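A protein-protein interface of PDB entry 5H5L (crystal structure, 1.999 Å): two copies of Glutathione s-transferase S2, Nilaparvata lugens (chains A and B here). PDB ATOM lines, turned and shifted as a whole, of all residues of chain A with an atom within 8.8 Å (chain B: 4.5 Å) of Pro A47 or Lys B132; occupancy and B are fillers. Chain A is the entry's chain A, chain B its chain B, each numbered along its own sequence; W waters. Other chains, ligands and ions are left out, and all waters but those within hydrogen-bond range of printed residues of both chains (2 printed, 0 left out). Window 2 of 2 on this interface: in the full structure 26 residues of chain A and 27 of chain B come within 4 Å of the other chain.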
ATOM      1  N   THR A   7      33.310  21.709  -1.284  1.00  0.00           N
ATOM      2  CA  THR A   7      33.435  22.938  -2.061  1.00  0.00           C
ATOM      3  C   THR A   7      32.477  24.000  -1.535  1.00  0.00           C
ATOM      4  O   THR A   7      31.257  23.801  -1.524  1.00  0.00           O
ATOM      5  CB  THR A   7      33.169  22.655  -3.546  1.00  0.00           C
ATOM      6  OG1 THR A   7      34.165  21.758  -4.022  1.00  0.00           O
ATOM      7  CG2 THR A   7      33.214  23.927  -4.380  1.00  0.00           C
ATOM      8  N   TRP A  39      33.983  31.592  -9.110  1.00  0.00           N
ATOM      9  CA  TRP A  39      32.663  31.007  -8.873  1.00  0.00           C
ATOM     10  C   TRP A  39      31.806  30.876 -10.132  1.00  0.00           C
ATOM     11  O   TRP A  39      31.028  29.910 -10.216  1.00  0.00           O
ATOM     12  CB  TRP A  39      31.926  31.829  -7.817  1.00  0.00           C
ATOM     13  CG  TRP A  39      30.504  31.429  -7.656  1.00  0.00           C
ATOM     14  CD1 TRP A  39      29.409  32.234  -7.777  1.00  0.00           C
ATOM     15  CD2 TRP A  39      30.012  30.113  -7.371  1.00  0.00           C
ATOM     16  NE1 TRP A  39      28.260  31.499  -7.568  1.00  0.00           N
ATOM     17  CE2 TRP A  39      28.611  30.197  -7.319  1.00  0.00           C
ATOM     18  CE3 TRP A  39      30.629  28.870  -7.122  1.00  0.00           C
ATOM     19  CZ2 TRP A  39      27.815  29.101  -7.031  1.00  0.00           C
ATOM     20  CZ3 TRP A  39      29.825  27.766  -6.858  1.00  0.00           C
ATOM     21  CH2 TRP A  39      28.441  27.889  -6.815  1.00  0.00           C
ATOM     22  N   ILE A  42      32.804  27.606 -11.534  1.00  0.00           N
ATOM     23  CA  ILE A  42      32.487  26.426 -10.732  1.00  0.00           C
ATOM     24  C   ILE A  42      30.984  26.203 -10.672  1.00  0.00           C
ATOM     25  O   ILE A  42      30.531  25.057 -10.557  1.00  0.00           O
ATOM     26  CB  ILE A  42      33.094  26.577  -9.323  1.00  0.00           C
ATOM     27  CG1 ILE A  42      34.632  26.630  -9.366  1.00  0.00           C
ATOM     28  CG2 ILE A  42      32.654  25.461  -8.431  1.00  0.00           C
ATOM     29  CD1 ILE A  42      35.285  25.390  -9.995  1.00  0.00           C
ATOM     30  N   LYS A  43      30.189  27.277 -10.771  1.00  0.00           N
ATOM     31  CA  LYS A  43      28.768  27.202 -10.437  1.00  0.00           C
ATOM     32  C   LYS A  43      28.039  26.176 -11.298  1.00  0.00           C
ATOM     33  O   LYS A  43      27.175  25.433 -10.807  1.00  0.00           O
ATOM     34  CB  LYS A  43      28.139  28.590 -10.582  1.00  0.00           C
ATOM     35  CG  LYS A  43      26.618  28.678 -10.448  1.00  0.00           C
ATOM     36  CD  LYS A  43      26.147  30.141 -10.692  1.00  0.00           C
ATOM     37  CE  LYS A  43      24.626  30.311 -10.574  1.00  0.00           C
ATOM     38  NZ  LYS A  43      24.146  30.217  -9.144  1.00  0.00           N
ATOM     39  N   SER A  44      28.381  26.108 -12.580  1.00  0.00           N
ATOM     40  CA  SER A  44      27.671  25.207 -13.484  1.00  0.00           C
ATOM     41  C   SER A  44      27.988  23.739 -13.221  1.00  0.00           C
ATOM     42  O   SER A  44      27.201  22.874 -13.613  1.00  0.00           O
ATOM     43  CB  SER A  44      28.009  25.555 -14.934  1.00  0.00           C
ATOM     44  OG  SER A  44      29.403  25.799 -15.059  1.00  0.00           O
ATOM     45  N   THR A  45      29.116  23.446 -12.568  1.00  0.00           N
ATOM     46  CA  THR A  45      29.492  22.084 -12.204  1.00  0.00           C
ATOM     47  C   THR A  45      28.743  21.576 -10.964  1.00  0.00           C
ATOM     48  O   THR A  45      28.809  20.377 -10.661  1.00  0.00           O
ATOM     49  CB  THR A  45      31.023  21.994 -11.955  1.00  0.00           C
ATOM     50  OG1 THR A  45      31.329  22.391 -10.618  1.00  0.00           O
ATOM     51  CG2 THR A  45      31.829  22.879 -12.909  1.00  0.00           C
ATOM     52  N   THR A  46      28.013  22.449 -10.240  1.00  0.00           N
ATOM     53  CA  THR A  46      27.351  21.981  -9.028  1.00  0.00           C
ATOM     54  C   THR A  46      25.965  21.434  -9.361  1.00  0.00           C
ATOM     55  O   THR A  46      25.388  21.781 -10.400  1.00  0.00           O
ATOM     56  CB  THR A  46      27.221  23.128  -8.026  1.00  0.00           C
ATOM     57  OG1 THR A  46      26.323  24.114  -8.553  1.00  0.00           O
ATOM     58  CG2 THR A  46      28.585  23.777  -7.720  1.00  0.00           C
ATOM     59  N   PRO A  47      25.384  20.600  -8.485  1.00  0.00           N
ATOM     60  CA  PRO A  47      24.080  19.987  -8.833  1.00  0.00           C
ATOM     61  C   PRO A  47      22.982  20.990  -9.138  1.00  0.00           C
ATOM     62  O   PRO A  47      22.263  20.837 -10.136  1.00  0.00           O
ATOM     63  CB  PRO A  47      23.752  19.138  -7.595  1.00  0.00           C
ATOM     64  CG  PRO A  47      25.141  18.695  -7.099  1.00  0.00           C
ATOM     65  CD  PRO A  47      25.972  19.987  -7.276  1.00  0.00           C
ATOM     66  N   TYR A  48      22.825  22.017  -8.305  1.00  0.00           N
ATOM     67  CA  TYR A  48      21.696  22.926  -8.429  1.00  0.00           C
ATOM     68  C   TYR A  48      22.143  24.380  -8.391  1.00  0.00           C
ATOM     69  O   TYR A  48      21.353  25.257  -8.048  1.00  0.00           O
ATOM     70  CB  TYR A  48      20.660  22.620  -7.343  1.00  0.00           C
ATOM     71  CG  TYR A  48      19.881  21.348  -7.637  1.00  0.00           C
ATOM     72  CD1 TYR A  48      18.761  21.387  -8.439  1.00  0.00           C
ATOM     73  CD2 TYR A  48      20.277  20.133  -7.122  1.00  0.00           C
ATOM     74  CE1 TYR A  48      18.045  20.264  -8.707  1.00  0.00           C
ATOM     75  CE2 TYR A  48      19.584  18.985  -7.402  1.00  0.00           C
ATOM     76  CZ  TYR A  48      18.480  19.064  -8.214  1.00  0.00           C
ATOM     77  OH  TYR A  48      17.782  17.951  -8.491  1.00  0.00           O
ATOM     78  N   GLY A  49      23.385  24.642  -8.770  1.00  0.00           N
ATOM     79  CA  GLY A  49      23.862  25.992  -8.931  1.00  0.00           C
ATOM     80  C   GLY A  49      24.350  26.669  -7.671  1.00  0.00           C
ATOM     81  O   GLY A  49      24.613  27.873  -7.703  1.00  0.00           O
ATOM     82  N   GLN A  50      24.488  25.941  -6.567  1.00  0.00           N
ATOM     83  CA  GLN A  50      24.859  26.557  -5.306  1.00  0.00           C
ATOM     84  C   GLN A  50      25.818  25.655  -4.566  1.00  0.00           C
ATOM     85  O   GLN A  50      25.987  24.483  -4.903  1.00  0.00           O
ATOM     86  CB  GLN A  50      23.642  26.840  -4.435  1.00  0.00           C
ATOM     87  CG  GLN A  50      22.688  27.927  -4.974  1.00  0.00           C
ATOM     88  CD  GLN A  50      21.915  28.603  -3.853  1.00  0.00           C
ATOM     89  OE1 GLN A  50      21.094  27.975  -3.188  1.00  0.00           O
ATOM     90  NE2 GLN A  50      22.204  29.880  -3.622  1.00  0.00           N
ATOM     91  N   VAL A  51      26.492  26.262  -3.601  1.00  0.00           N
ATOM     92  CA  VAL A  51      27.365  25.577  -2.659  1.00  0.00           C
ATOM     93  C   VAL A  51      26.815  25.831  -1.261  1.00  0.00           C
ATOM     94  O   VAL A  51      26.098  26.819  -1.019  1.00  0.00           O
ATOM     95  CB  VAL A  51      28.830  26.032  -2.817  1.00  0.00           C
ATOM     96  CG1 VAL A  51      29.363  25.464  -4.116  1.00  0.00           C
ATOM     97  CG2 VAL A  51      28.956  27.619  -2.784  1.00  0.00           C
ATOM     98  N   PRO A  52      27.163  24.997  -0.299  1.00  0.00           N
ATOM     99  CA  PRO A  52      28.170  23.950  -0.306  1.00  0.00           C
ATOM    100  C   PRO A  52      27.760  22.703  -1.076  1.00  0.00           C
ATOM    101  O   PRO A  52      26.569  22.378  -1.175  1.00  0.00           O
ATOM    102  CB  PRO A  52      28.332  23.633   1.181  1.00  0.00           C
ATOM    103  CG  PRO A  52      27.068  23.934   1.766  1.00  0.00           C
ATOM    104  CD  PRO A  52      26.527  25.119   1.023  1.00  0.00           C
ATOM    105  N   VAL A  53      28.786  22.029  -1.600  1.00  0.00           N
ATOM    106  CA  VAL A  53      28.713  20.694  -2.177  1.00  0.00           C
ATOM    107  C   VAL A  53      29.737  19.828  -1.453  1.00  0.00           C
ATOM    108  O   VAL A  53      30.902  20.218  -1.331  1.00  0.00           O
ATOM    109  CB  VAL A  53      29.009  20.708  -3.687  1.00  0.00           C
ATOM    110  CG1 VAL A  53      28.985  19.244  -4.272  1.00  0.00           C
ATOM    111  CG2 VAL A  53      28.018  21.562  -4.368  1.00  0.00           C
ATOM    112  N   LEU A  54      29.315  18.665  -0.967  1.00  0.00           N
ATOM    113  CA  LEU A  54      30.231  17.710  -0.377  1.00  0.00           C
ATOM    114  C   LEU A  54      30.281  16.497  -1.300  1.00  0.00           C
ATOM    115  O   LEU A  54      29.246  15.886  -1.574  1.00  0.00           O
ATOM    116  CB  LEU A  54      29.785  17.317   1.022  1.00  0.00           C
ATOM    117  CG  LEU A  54      30.700  16.311   1.683  1.00  0.00           C
ATOM    118  CD1 LEU A  54      31.956  17.003   2.171  1.00  0.00           C
ATOM    119  CD2 LEU A  54      29.978  15.635   2.846  1.00  0.00           C
ATOM    120  N   GLU A  55      31.473  16.167  -1.790  1.00  0.00           N
ATOM    121  CA  GLU A  55      31.649  14.987  -2.630  1.00  0.00           C
ATOM    122  C   GLU A  55      32.086  13.849  -1.737  1.00  0.00           C
ATOM    123  O   GLU A  55      33.063  13.969  -0.997  1.00  0.00           O
ATOM    124  CB  GLU A  55      32.680  15.200  -3.729  1.00  0.00           C
ATOM    125  CG  GLU A  55      32.199  16.061  -4.822  1.00  0.00           C
ATOM    126  CD  GLU A  55      33.311  16.402  -5.783  1.00  0.00           C
ATOM    127  OE1 GLU A  55      33.356  17.560  -6.245  1.00  0.00           O
ATOM    128  OE2 GLU A  55      34.150  15.512  -6.039  1.00  0.00           O
ATOM    129  N   LYS A  59      30.755  11.233  -5.199  1.00  0.00           N
ATOM    130  CA  LYS A  59      29.353  11.572  -5.420  1.00  0.00           C
ATOM    131  C   LYS A  59      29.049  12.952  -4.844  1.00  0.00           C
ATOM    132  O   LYS A  59      29.269  13.201  -3.655  1.00  0.00           O
ATOM    133  CB  LYS A  59      28.427  10.552  -4.773  1.00  0.00           C
ATOM    134  CG  LYS A  59      28.735   9.074  -5.126  1.00  0.00           C
ATOM    135  CD  LYS A  59      27.501   8.170  -4.980  1.00  0.00           C
ATOM    136  CE  LYS A  59      27.877   6.698  -4.852  1.00  0.00           C
ATOM    137  NZ  LYS A  59      28.167   6.323  -3.437  1.00  0.00           N
ATOM    138  N   GLN A  60      28.470  13.804  -5.667  1.00  0.00           N
ATOM    139  CA  GLN A  60      28.133  15.161  -5.263  1.00  0.00           C
ATOM    140  C   GLN A  60      26.838  15.155  -4.453  1.00  0.00           C
ATOM    141  O   GLN A  60      25.802  14.688  -4.924  1.00  0.00           O
ATOM    142  CB  GLN A  60      27.985  16.056  -6.480  1.00  0.00           C
ATOM    143  CG  GLN A  60      29.310  16.461  -7.109  1.00  0.00           C
ATOM    144  CD  GLN A  60      29.127  17.431  -8.258  1.00  0.00           C
ATOM    145  OE1 GLN A  60      28.088  17.432  -8.935  1.00  0.00           O
ATOM    146  NE2 GLN A  60      30.135  18.255  -8.490  1.00  0.00           N
ATOM    147  N   VAL A  61      26.904  15.677  -3.238  1.00  0.00           N
ATOM    148  CA  VAL A  61      25.729  15.907  -2.404  1.00  0.00           C
ATOM    149  C   VAL A  61      25.684  17.379  -2.009  1.00  0.00           C
ATOM    150  O   VAL A  61      26.693  17.932  -1.568  1.00  0.00           O
ATOM    151  CB  VAL A  61      25.768  15.016  -1.152  1.00  0.00           C
ATOM    152  CG1 VAL A  61      24.406  15.126  -0.419  1.00  0.00           C
ATOM    153  CG2 VAL A  61      26.055  13.580  -1.565  1.00  0.00           C
ATOM    154  N   CYS A  62      24.524  18.005  -2.167  1.00  0.00           N
ATOM    155  CA  CYS A  62      24.391  19.372  -1.680  1.00  0.00           C
ATOM    156  C   CYS A  62      23.443  19.426  -0.486  1.00  0.00           C
ATOM    157  O   CYS A  62      22.976  18.399   0.016  1.00  0.00           O
ATOM    158  CB  CYS A  62      23.934  20.297  -2.799  1.00  0.00           C
ATOM    159  SG  CYS A  62      22.405  19.795  -3.462  1.00  0.00           S
ATOM    160  N   GLN A  63      23.250  20.652   0.002  1.00  0.00           N
ATOM    161  CA  GLN A  63      22.321  21.041   1.065  1.00  0.00           C
ATOM    162  C   GLN A  63      22.948  20.916   2.437  1.00  0.00           C
ATOM    163  O   GLN A  63      23.067  19.811   3.001  1.00  0.00           O
ATOM    164  CB  GLN A  63      21.020  20.249   1.013  1.00  0.00           C
ATOM    165  CG  GLN A  63      20.193  20.604  -0.206  1.00  0.00           C
ATOM    166  CD  GLN A  63      19.826  22.075  -0.247  1.00  0.00           C
ATOM    167  OE1 GLN A  63      19.837  22.756   0.783  1.00  0.00           O
ATOM    168  NE2 GLN A  63      19.537  22.581  -1.433  1.00  0.00           N
ATOM    169  N   PHE B 128      14.593  25.051 -14.650  1.00  0.00           N
ATOM    170  CA  PHE B 128      15.882  24.718 -14.055  1.00  0.00           C
ATOM    171  C   PHE B 128      15.724  23.581 -13.054  1.00  0.00           C
ATOM    172  O   PHE B 128      16.366  22.527 -13.173  1.00  0.00           O
ATOM    173  CB  PHE B 128      16.504  25.949 -13.394  1.00  0.00           C
ATOM    174  CG  PHE B 128      17.799  25.661 -12.686  1.00  0.00           C
ATOM    175  CD1 PHE B 128      18.994  25.720 -13.365  1.00  0.00           C
ATOM    176  CD2 PHE B 128      17.807  25.273 -11.354  1.00  0.00           C
ATOM    177  CE1 PHE B 128      20.188  25.437 -12.727  1.00  0.00           C
ATOM    178  CE2 PHE B 128      18.992  24.989 -10.710  1.00  0.00           C
ATOM    179  CZ  PHE B 128      20.183  25.067 -11.400  1.00  0.00           C
ATOM    180  N   TYR B 129      14.830  23.756 -12.077  1.00  0.00           N
ATOM    181  CA  TYR B 129      14.644  22.725 -11.054  1.00  0.00           C
ATOM    182  C   TYR B 129      13.916  21.514 -11.605  1.00  0.00           C
ATOM    183  O   TYR B 129      14.308  20.373 -11.341  1.00  0.00           O
ATOM    184  CB  TYR B 129      13.869  23.275  -9.843  1.00  0.00           C
ATOM    185  CG  TYR B 129      14.734  24.148  -8.969  1.00  0.00           C
ATOM    186  CD1 TYR B 129      15.565  23.605  -8.002  1.00  0.00           C
ATOM    187  CD2 TYR B 129      14.740  25.507  -9.130  1.00  0.00           C
ATOM    188  CE1 TYR B 129      16.373  24.421  -7.217  1.00  0.00           C
ATOM    189  CE2 TYR B 129      15.544  26.318  -8.372  1.00  0.00           C
ATOM    190  CZ  TYR B 129      16.348  25.781  -7.408  1.00  0.00           C
ATOM    191  OH  TYR B 129      17.151  26.615  -6.673  1.00  0.00           O
ATOM    192  N   PHE B 130      12.841  21.725 -12.367  1.00  0.00           N
ATOM    193  CA  PHE B 130      12.014  20.571 -12.704  1.00  0.00           C
ATOM    194  C   PHE B 130      12.666  19.654 -13.730  1.00  0.00           C
ATOM    195  O   PHE B 130      12.390  18.451 -13.706  1.00  0.00           O
ATOM    196  CB  PHE B 130      10.653  21.009 -13.188  1.00  0.00           C
ATOM    197  CG  PHE B 130       9.735  21.437 -12.081  1.00  0.00           C
ATOM    198  CD1 PHE B 130      10.243  21.988 -10.907  1.00  0.00           C
ATOM    199  CD2 PHE B 130       8.379  21.284 -12.210  1.00  0.00           C
ATOM    200  CE1 PHE B 130       9.397  22.378  -9.886  1.00  0.00           C
ATOM    201  CE2 PHE B 130       7.514  21.689 -11.207  1.00  0.00           C
ATOM    202  CZ  PHE B 130       8.012  22.223 -10.044  1.00  0.00           C
ATOM    203  N   ASN B 131      13.495  20.174 -14.647  1.00  0.00           N
ATOM    204  CA  ASN B 131      14.220  19.263 -15.542  1.00  0.00           C
ATOM    205  C   ASN B 131      15.147  18.363 -14.725  1.00  0.00           C
ATOM    206  O   ASN B 131      15.238  17.154 -14.966  1.00  0.00           O
ATOM    207  CB  ASN B 131      15.031  20.030 -16.590  1.00  0.00           C
ATOM    208  CG  ASN B 131      14.195  20.532 -17.772  1.00  0.00           C
ATOM    209  OD1 ASN B 131      13.277  19.872 -18.235  1.00  0.00           O
ATOM    210  ND2 ASN B 131      14.544  21.694 -18.263  1.00  0.00           N
ATOM    211  N   LYS B 132      15.825  18.931 -13.720  1.00  0.00           N
ATOM    212  CA  LYS B 132      16.695  18.108 -12.883  1.00  0.00           C
ATOM    213  C   LYS B 132      15.895  17.109 -12.052  1.00  0.00           C
ATOM    214  O   LYS B 132      16.295  15.945 -11.934  1.00  0.00           O
ATOM    215  CB  LYS B 132      17.551  19.000 -11.993  1.00  0.00           C
ATOM    216  CG  LYS B 132      18.747  19.616 -12.753  1.00  0.00           C
ATOM    217  CD  LYS B 132      19.134  20.952 -12.146  1.00  0.00           C
ATOM    218  CE  LYS B 132      20.306  21.580 -12.864  1.00  0.00           C
ATOM    219  NZ  LYS B 132      21.585  20.815 -12.660  1.00  0.00           N
ATOM    220  N   PHE B 133      14.786  17.551 -11.435  1.00  0.00           N
ATOM    221  CA  PHE B 133      13.927  16.633 -10.688  1.00  0.00           C
ATOM    222  C   PHE B 133      13.437  15.520 -11.600  1.00  0.00           C
ATOM    223  O   PHE B 133      13.428  14.335 -11.232  1.00  0.00           O
ATOM    224  CB  PHE B 133      12.701  17.363 -10.113  1.00  0.00           C
ATOM    225  CG  PHE B 133      12.999  18.408  -9.061  1.00  0.00           C
ATOM    226  CD1 PHE B 133      14.211  18.470  -8.390  1.00  0.00           C
ATOM    227  CD2 PHE B 133      12.025  19.339  -8.744  1.00  0.00           C
ATOM    228  CE1 PHE B 133      14.435  19.441  -7.431  1.00  0.00           C
ATOM    229  CE2 PHE B 133      12.267  20.322  -7.817  1.00  0.00           C
ATOM    230  CZ  PHE B 133      13.468  20.354  -7.152  1.00  0.00           C
ATOM    231  N   ASN B 134      12.970  15.907 -12.785  1.00  0.00           N
ATOM    232  CA  ASN B 134      12.481  14.942 -13.773  1.00  0.00           C
ATOM    233  C   ASN B 134      13.557  13.900 -14.110  1.00  0.00           C
ATOM    234  O   ASN B 134      13.312  12.693 -14.049  1.00  0.00           O
ATOM    235  CB  ASN B 134      12.037  15.721 -15.012  1.00  0.00           C
ATOM    236  CG  ASN B 134      11.068  14.947 -15.894  1.00  0.00           C
ATOM    237  OD1 ASN B 134      10.172  14.238 -15.436  1.00  0.00           O
ATOM    238  ND2 ASN B 134      11.243  15.100 -17.178  1.00  0.00           N
ATOM    239  N   ASP B 135      14.767  14.360 -14.423  1.00  0.00           N
ATOM    240  CA  ASP B 135      15.882  13.466 -14.731  1.00  0.00           C
ATOM    241  C   ASP B 135      16.253  12.624 -13.513  1.00  0.00           C
ATOM    242  O   ASP B 135      16.545  11.428 -13.627  1.00  0.00           O
ATOM    243  CB  ASP B 135      17.052  14.336 -15.225  1.00  0.00           C
ATOM    244  CG  ASP B 135      18.404  13.601 -15.333  1.00  0.00           C
ATOM    245  OD1 ASP B 135      18.698  13.050 -16.413  1.00  0.00           O
ATOM    246  OD2 ASP B 135      19.216  13.654 -14.372  1.00  0.00           O
ATOM    247  N   HIS B 136      16.189  13.219 -12.325  1.00  0.00           N
ATOM    248  CA  HIS B 136      16.549  12.479 -11.118  1.00  0.00           C
ATOM    249  C   HIS B 136      15.557  11.368 -10.852  1.00  0.00           C
ATOM    250  O   HIS B 136      15.951  10.237 -10.549  1.00  0.00           O
ATOM    251  CB  HIS B 136      16.619  13.447  -9.939  1.00  0.00           C
ATOM    252  CG  HIS B 136      17.080  12.825  -8.671  1.00  0.00           C
ATOM    253  ND1 HIS B 136      18.407  12.743  -8.330  1.00  0.00           N
ATOM    254  CD2 HIS B 136      16.385  12.288  -7.638  1.00  0.00           C
ATOM    255  CE1 HIS B 136      18.516  12.177  -7.138  1.00  0.00           C
ATOM    256  NE2 HIS B 136      17.302  11.904  -6.689  1.00  0.00           N
HETATM  257  O   HOH W   1      19.555  25.930  -6.123  1.00  0.00           O
HETATM  258  O   HOH W   2      19.312  15.637  -8.069  1.00  0.00           O
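The backbone carbonyl oxygen (O) of Pro A47 is in hydrogen-bond range of the side-chain amino group (NZ) of Lys B132, at 2.6 Å.
Among the printed residues, pairs that only touch across the chains: Tyr A48 with Phe B128 (3.6 Å), Tyr A48 with Tyr B129 (3.9 Å), Tyr A48 with Lys B132 (3.6 Å) and Tyr A48 with Phe B133 (3.6 Å).
Lys B132 touches just these residues of chain A: Pro A47 and Tyr A48. Of the printed residues of chain A, Phe B133 touches Tyr A48 (3.6 Å). Printed residues of chain B within 4 Å of Tyr A48: Phe B128 (3.6 Å), Tyr B129 (3.9 Å), Lys B132 (3.6 Å) and Phe B133 (3.6 Å). Of the printed residues of chain A, Phe B128 touches Tyr A48 (3.6 Å). Of the printed residues of chain A, Tyr B129 touches Tyr A48 (3.9 Å). The nearest residue of chain A that does not touch Lys B132 is Thr A46 (4.5 Å).
Of the 9 printed residues of chain B, 4 touch a printed residue of chain A. Hydrophobic or aromatic side chains of chain B that line the printed part of chain A: Phe B128, Tyr B129 and Phe B133. Among the printed residues, 5 pairs touch across the chains.
No position is printed for both chains.
Water W1 bridges the side-chain hydroxyl of Tyr B129 and the backbone carbonyl oxygen of Tyr A48. Water W2 lies within hydrogen-bond range of the side-chain hydroxyl (OH) of Tyr A48 (2.8 Å) and a ring nitrogen (ND1) of His B136 (3.0 Å).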
